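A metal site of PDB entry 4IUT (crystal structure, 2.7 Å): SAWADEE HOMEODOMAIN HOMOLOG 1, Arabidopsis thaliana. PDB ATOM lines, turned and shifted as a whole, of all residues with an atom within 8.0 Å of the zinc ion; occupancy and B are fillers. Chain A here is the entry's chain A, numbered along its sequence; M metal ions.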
ATOM      1  N   VAL A  63       6.117 -20.162  -2.180  1.00  0.00           N
ATOM      2  CA  VAL A  63       7.042 -19.837  -3.259  1.00  0.00           C
ATOM      3  C   VAL A  63       6.312 -19.770  -4.595  1.00  0.00           C
ATOM      4  O   VAL A  63       5.652 -20.729  -4.999  1.00  0.00           O
ATOM      5  CB  VAL A  63       8.171 -20.865  -3.348  1.00  0.00           C
ATOM      6  CG1 VAL A  63       9.185 -20.443  -4.408  1.00  0.00           C
ATOM      7  CG2 VAL A  63       8.849 -21.018  -1.999  1.00  0.00           C
ATOM      8  N   GLU A  64       6.424 -18.642  -5.284  1.00  0.00           N
ATOM      9  CA  GLU A  64       5.845 -18.495  -6.610  1.00  0.00           C
ATOM     10  C   GLU A  64       6.651 -19.292  -7.632  1.00  0.00           C
ATOM     11  O   GLU A  64       7.860 -19.473  -7.477  1.00  0.00           O
ATOM     12  CB  GLU A  64       5.787 -17.025  -7.038  1.00  0.00           C
ATOM     13  CG  GLU A  64       4.623 -16.244  -6.467  1.00  0.00           C
ATOM     14  CD  GLU A  64       4.362 -14.957  -7.223  1.00  0.00           C
ATOM     15  OE1 GLU A  64       4.174 -13.905  -6.580  1.00  0.00           O
ATOM     16  OE2 GLU A  64       4.337 -15.002  -8.480  1.00  0.00           O
ATOM     17  N   PRO A  65       5.977 -19.774  -8.684  1.00  0.00           N
ATOM     18  CA  PRO A  65       6.663 -20.517  -9.755  1.00  0.00           C
ATOM     19  C   PRO A  65       7.854 -19.734 -10.293  1.00  0.00           C
ATOM     20  O   PRO A  65       8.868 -20.339 -10.645  1.00  0.00           O
ATOM     21  CB  PRO A  65       5.584 -20.658 -10.822  1.00  0.00           C
ATOM     22  CG  PRO A  65       4.306 -20.649 -10.058  1.00  0.00           C
ATOM     23  CD  PRO A  65       4.527 -19.695  -8.912  1.00  0.00           C
ATOM     24  N   SER A  66       7.736 -18.410 -10.362  1.00  0.00           N
ATOM     25  CA  SER A  66       8.793 -17.574 -10.910  1.00  0.00           C
ATOM     26  C   SER A  66      10.072 -17.611 -10.061  1.00  0.00           C
ATOM     27  O   SER A  66      11.161 -17.339 -10.559  1.00  0.00           O
ATOM     28  CB  SER A  66       8.318 -16.127 -11.078  1.00  0.00           C
ATOM     29  OG  SER A  66       7.985 -15.563  -9.822  1.00  0.00           O
ATOM     30  N   GLU A  67       9.925 -17.954  -8.786  1.00  0.00           N
ATOM     31  CA  GLU A  67      11.052 -17.955  -7.868  1.00  0.00           C
ATOM     32  C   GLU A  67      11.483 -19.350  -7.416  1.00  0.00           C
ATOM     33  O   GLU A  67      12.253 -19.491  -6.456  1.00  0.00           O
ATOM     34  CB  GLU A  67      10.764 -17.065  -6.647  1.00  0.00           C
ATOM     35  CG  GLU A  67       9.424 -17.325  -5.994  1.00  0.00           C
ATOM     36  CD  GLU A  67       9.217 -16.466  -4.754  1.00  0.00           C
ATOM     37  OE1 GLU A  67      10.150 -15.742  -4.370  1.00  0.00           O
ATOM     38  OE2 GLU A  67       8.113 -16.533  -4.172  1.00  0.00           O
ATOM     39  N   CYS A  68      11.000 -20.378  -8.102  1.00  0.00           N
ATOM     40  CA  CYS A  68      11.326 -21.767  -7.763  1.00  0.00           C
ATOM     41  C   CYS A  68      12.831 -22.027  -7.748  1.00  0.00           C
ATOM     42  O   CYS A  68      13.277 -23.105  -7.343  1.00  0.00           O
ATOM     43  CB  CYS A  68      10.674 -22.711  -8.768  1.00  0.00           C
ATOM     44  SG  CYS A  68      11.478 -22.685 -10.383  1.00  0.00           S
ATOM     45  N   GLY A  69      13.603 -21.052  -8.212  1.00  0.00           N
ATOM     46  CA  GLY A  69      15.034 -21.209  -8.331  1.00  0.00           C
ATOM     47  C   GLY A  69      15.809 -20.839  -7.074  1.00  0.00           C
ATOM     48  O   GLY A  69      17.023 -21.036  -7.011  1.00  0.00           O
ATOM     49  N   ILE A  97      16.791 -31.968  -6.374  1.00  0.00           N
ATOM     50  CA  ILE A  97      15.839 -31.194  -7.162  1.00  0.00           C
ATOM     51  C   ILE A  97      15.894 -31.562  -8.631  1.00  0.00           C
ATOM     52  O   ILE A  97      16.954 -31.462  -9.262  1.00  0.00           O
ATOM     53  CB  ILE A  97      16.106 -29.687  -7.058  1.00  0.00           C
ATOM     54  CG1 ILE A  97      16.173 -29.247  -5.602  1.00  0.00           C
ATOM     55  CG2 ILE A  97      15.026 -28.909  -7.799  1.00  0.00           C
ATOM     56  CD1 ILE A  97      16.489 -27.782  -5.439  1.00  0.00           C
ATOM     57  N   LYS A  98      14.774 -31.979  -9.188  1.00  0.00           N
ATOM     58  CA  LYS A  98      14.701 -32.292 -10.596  1.00  0.00           C
ATOM     59  C   LYS A  98      13.932 -31.189 -11.327  1.00  0.00           C
ATOM     60  O   LYS A  98      12.706 -31.129 -11.270  1.00  0.00           O
ATOM     61  CB  LYS A  98      14.044 -33.662 -10.819  1.00  0.00           C
ATOM     62  CG  LYS A  98      13.974 -34.079 -12.274  1.00  0.00           C
ATOM     63  CD  LYS A  98      13.485 -35.508 -12.418  1.00  0.00           C
ATOM     64  CE  LYS A  98      13.021 -35.763 -13.830  1.00  0.00           C
ATOM     65  NZ  LYS A  98      12.674 -37.201 -13.991  1.00  0.00           N
ATOM     66  N   ARG A  99      14.672 -30.321 -12.000  1.00  0.00           N
ATOM     67  CA  ARG A  99      14.102 -29.145 -12.651  1.00  0.00           C
ATOM     68  C   ARG A  99      13.294 -29.502 -13.898  1.00  0.00           C
ATOM     69  O   ARG A  99      13.724 -30.303 -14.728  1.00  0.00           O
ATOM     70  CB  ARG A  99      15.207 -28.151 -13.006  1.00  0.00           C
ATOM     71  CG  ARG A  99      15.977 -27.610 -11.817  1.00  0.00           C
ATOM     72  CD  ARG A  99      15.065 -26.808 -10.897  1.00  0.00           C
ATOM     73  NE  ARG A  99      15.831 -26.102  -9.867  1.00  0.00           N
ATOM     74  CZ  ARG A  99      15.288 -25.363  -8.904  1.00  0.00           C
ATOM     75  NH1 ARG A  99      13.969 -25.222  -8.833  1.00  0.00           N
ATOM     76  NH2 ARG A  99      16.059 -24.756  -8.020  1.00  0.00           N
ATOM     77  N   GLY A 100      12.119 -28.898 -14.011  1.00  0.00           N
ATOM     78  CA  GLY A 100      11.259 -29.101 -15.169  1.00  0.00           C
ATOM     79  C   GLY A 100      11.198 -27.863 -16.044  1.00  0.00           C
ATOM     80  O   GLY A 100      11.773 -26.826 -15.706  1.00  0.00           O
ATOM     81  N   ILE A 101      10.528 -27.972 -17.180  1.00  0.00           N
ATOM     82  CA  ILE A 101      10.327 -26.832 -18.056  1.00  0.00           C
ATOM     83  C   ILE A 101       8.963 -26.221 -17.802  1.00  0.00           C
ATOM     84  O   ILE A 101       7.942 -26.898 -17.924  1.00  0.00           O
ATOM     85  CB  ILE A 101      10.422 -27.219 -19.555  1.00  0.00           C
ATOM     86  CG1 ILE A 101      11.001 -28.623 -19.723  1.00  0.00           C
ATOM     87  CG2 ILE A 101      11.234 -26.198 -20.327  1.00  0.00           C
ATOM     88  CD1 ILE A 101       9.952 -29.696 -19.884  1.00  0.00           C
ATOM     89  N   HIS A 102       8.947 -24.949 -17.431  1.00  0.00           N
ATOM     90  CA  HIS A 102       7.689 -24.267 -17.140  1.00  0.00           C
ATOM     91  C   HIS A 102       7.863 -22.759 -17.108  1.00  0.00           C
ATOM     92  O   HIS A 102       8.951 -22.246 -17.358  1.00  0.00           O
ATOM     93  CB  HIS A 102       7.129 -24.743 -15.793  1.00  0.00           C
ATOM     94  CG  HIS A 102       7.949 -24.325 -14.621  1.00  0.00           C
ATOM     95  ND1 HIS A 102       7.809 -23.091 -14.014  1.00  0.00           N
ATOM     96  CD2 HIS A 102       8.931 -24.973 -13.933  1.00  0.00           C
ATOM     97  CE1 HIS A 102       8.663 -23.005 -13.016  1.00  0.00           C
ATOM     98  NE2 HIS A 102       9.348 -24.129 -12.941  1.00  0.00           N
ATOM     99  N   ASP A 103       6.787 -22.062 -16.782  1.00  0.00           N
ATOM    100  CA  ASP A 103       6.780 -20.603 -16.798  1.00  0.00           C
ATOM    101  C   ASP A 103       6.232 -20.033 -15.496  1.00  0.00           C
ATOM    102  O   ASP A 103       6.155 -20.716 -14.474  1.00  0.00           O
ATOM    103  CB  ASP A 103       5.956 -20.097 -17.984  1.00  0.00           C
ATOM    104  CG  ASP A 103       4.523 -20.583 -17.931  1.00  0.00           C
ATOM    105  OD1 ASP A 103       4.236 -21.520 -17.152  1.00  0.00           O
ATOM    106  OD2 ASP A 103       3.686 -20.050 -18.683  1.00  0.00           O
ATOM    107  N   ARG A 106       2.804 -21.892 -13.460  1.00  0.00           N
ATOM    108  CA  ARG A 106       2.850 -23.088 -12.622  1.00  0.00           C
ATOM    109  C   ARG A 106       4.214 -23.772 -12.670  1.00  0.00           C
ATOM    110  O   ARG A 106       4.803 -23.912 -13.750  1.00  0.00           O
ATOM    111  CB  ARG A 106       1.756 -24.068 -13.048  1.00  0.00           C
ATOM    112  CG  ARG A 106       1.815 -25.440 -12.392  1.00  0.00           C
ATOM    113  CD  ARG A 106       1.069 -25.483 -11.079  1.00  0.00           C
ATOM    114  NE  ARG A 106       0.516 -26.807 -10.825  1.00  0.00           N
ATOM    115  CZ  ARG A 106      -0.126 -27.156  -9.711  1.00  0.00           C
ATOM    116  NH1 ARG A 106      -0.597 -28.392  -9.580  1.00  0.00           N
ATOM    117  NH2 ARG A 106      -0.311 -26.266  -8.749  1.00  0.00           N
ATOM    118  N   CYS A 107       4.710 -24.187 -11.515  1.00  0.00           N
ATOM    119  CA  CYS A 107       5.990 -24.887 -11.436  1.00  0.00           C
ATOM    120  C   CYS A 107       5.774 -26.387 -11.468  1.00  0.00           C
ATOM    121  O   CYS A 107       4.895 -26.914 -10.774  1.00  0.00           O
ATOM    122  CB  CYS A 107       6.747 -24.493 -10.168  1.00  0.00           C
ATOM    123  SG  CYS A 107       8.143 -25.570  -9.772  1.00  0.00           S
ATOM    124  N   ASN A 108       6.568 -27.083 -12.272  1.00  0.00           N
ATOM    125  CA  ASN A 108       6.483 -28.537 -12.378  1.00  0.00           C
ATOM    126  C   ASN A 108       7.752 -29.242 -11.929  1.00  0.00           C
ATOM    127  O   ASN A 108       7.916 -30.443 -12.161  1.00  0.00           O
ATOM    128  CB  ASN A 108       6.096 -28.958 -13.791  1.00  0.00           C
ATOM    129  CG  ASN A 108       7.096 -28.499 -14.829  1.00  0.00           C
ATOM    130  OD1 ASN A 108       7.880 -27.579 -14.595  1.00  0.00           O
ATOM    131  ND2 ASN A 108       7.064 -29.126 -15.997  1.00  0.00           N
ATOM    132  N   CYS A 109       8.657 -28.503 -11.294  1.00  0.00           N
ATOM    133  CA  CYS A 109       9.866 -29.096 -10.737  1.00  0.00           C
ATOM    134  C   CYS A 109       9.504 -30.080  -9.632  1.00  0.00           C
ATOM    135  O   CYS A 109       8.478 -29.915  -8.962  1.00  0.00           O
ATOM    136  CB  CYS A 109      10.792 -28.009 -10.187  1.00  0.00           C
ATOM    137  SG  CYS A 109      11.546 -26.976 -11.460  1.00  0.00           S
ATOM    138  N   VAL A 110      10.329 -31.101  -9.456  1.00  0.00           N
ATOM    139  CA  VAL A 110      10.069 -32.117  -8.452  1.00  0.00           C
ATOM    140  C   VAL A 110      11.163 -32.137  -7.386  1.00  0.00           C
ATOM    141  O   VAL A 110      12.312 -32.433  -7.662  1.00  0.00           O
ATOM    142  CB  VAL A 110       9.949 -33.517  -9.086  1.00  0.00           C
ATOM    143  CG1 VAL A 110       9.683 -34.567  -8.004  1.00  0.00           C
ATOM    144  CG2 VAL A 110       8.842 -33.533 -10.125  1.00  0.00           C
ATOM    145  N   PHE A 111      10.765 -31.811  -6.158  1.00  0.00           N
ATOM    146  CA  PHE A 111      11.700 -31.749  -5.039  1.00  0.00           C
ATOM    147  C   PHE A 111      11.606 -33.007  -4.189  1.00  0.00           C
ATOM    148  O   PHE A 111      10.539 -33.314  -3.663  1.00  0.00           O
ATOM    149  CB  PHE A 111      11.412 -30.523  -4.166  1.00  0.00           C
ATOM    150  CG  PHE A 111      11.304 -29.227  -4.938  1.00  0.00           C
ATOM    151  CD1 PHE A 111      12.290 -28.267  -4.847  1.00  0.00           C
ATOM    152  CD2 PHE A 111      10.200 -28.972  -5.747  1.00  0.00           C
ATOM    153  CE1 PHE A 111      12.196 -27.087  -5.547  1.00  0.00           C
ATOM    154  CE2 PHE A 111      10.106 -27.792  -6.457  1.00  0.00           C
ATOM    155  CZ  PHE A 111      11.098 -26.841  -6.356  1.00  0.00           C
ATOM    156  N   LEU A 126       6.311 -27.566  -5.945  1.00  0.00           N
ATOM    157  CA  LEU A 126       6.313 -26.260  -5.300  1.00  0.00           C
ATOM    158  C   LEU A 126       5.015 -26.011  -4.529  1.00  0.00           C
ATOM    159  O   LEU A 126       5.026 -25.417  -3.453  1.00  0.00           O
ATOM    160  CB  LEU A 126       6.539 -25.156  -6.339  1.00  0.00           C
ATOM    161  CG  LEU A 126       7.239 -23.895  -5.832  1.00  0.00           C
ATOM    162  CD1 LEU A 126       8.640 -24.229  -5.353  1.00  0.00           C
ATOM    163  CD2 LEU A 126       7.278 -22.832  -6.918  1.00  0.00           C
HETATM  164 ZN    ZN M   1      10.292 -24.804 -10.952  1.00  0.00          ZN
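The zinc ion is bound by NE2 of His 102 (2.3 Å). SG of Cys 68 binds the zinc ion (2.5 Å). The zinc ion is bound by the side-chain sulfur (SG) of Cys 109 (2.6 Å). SG of Cys 107 is bound to the zinc ion (2.6 Å). The zinc ion has four donor atoms within binding distance.
Along chain A the residues within 4 Å of the zinc ion span positions 68 to 109.
ND1 of His 102 is in hydrogen-bond range of O of Arg 106 (3.1 Å). O of Cys 68 lies within hydrogen-bond range of NH1 of Arg 99 (2.7 Å). The backbone carbonyl oxygen of Pro 65 sits close to the side-chain sulfur of Cys 68, at 3.5 Å. The side-chain sulfur (SG) of Cys 109 sits close to the backbone NH (N) of Gly 100, 3.2 Å away.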
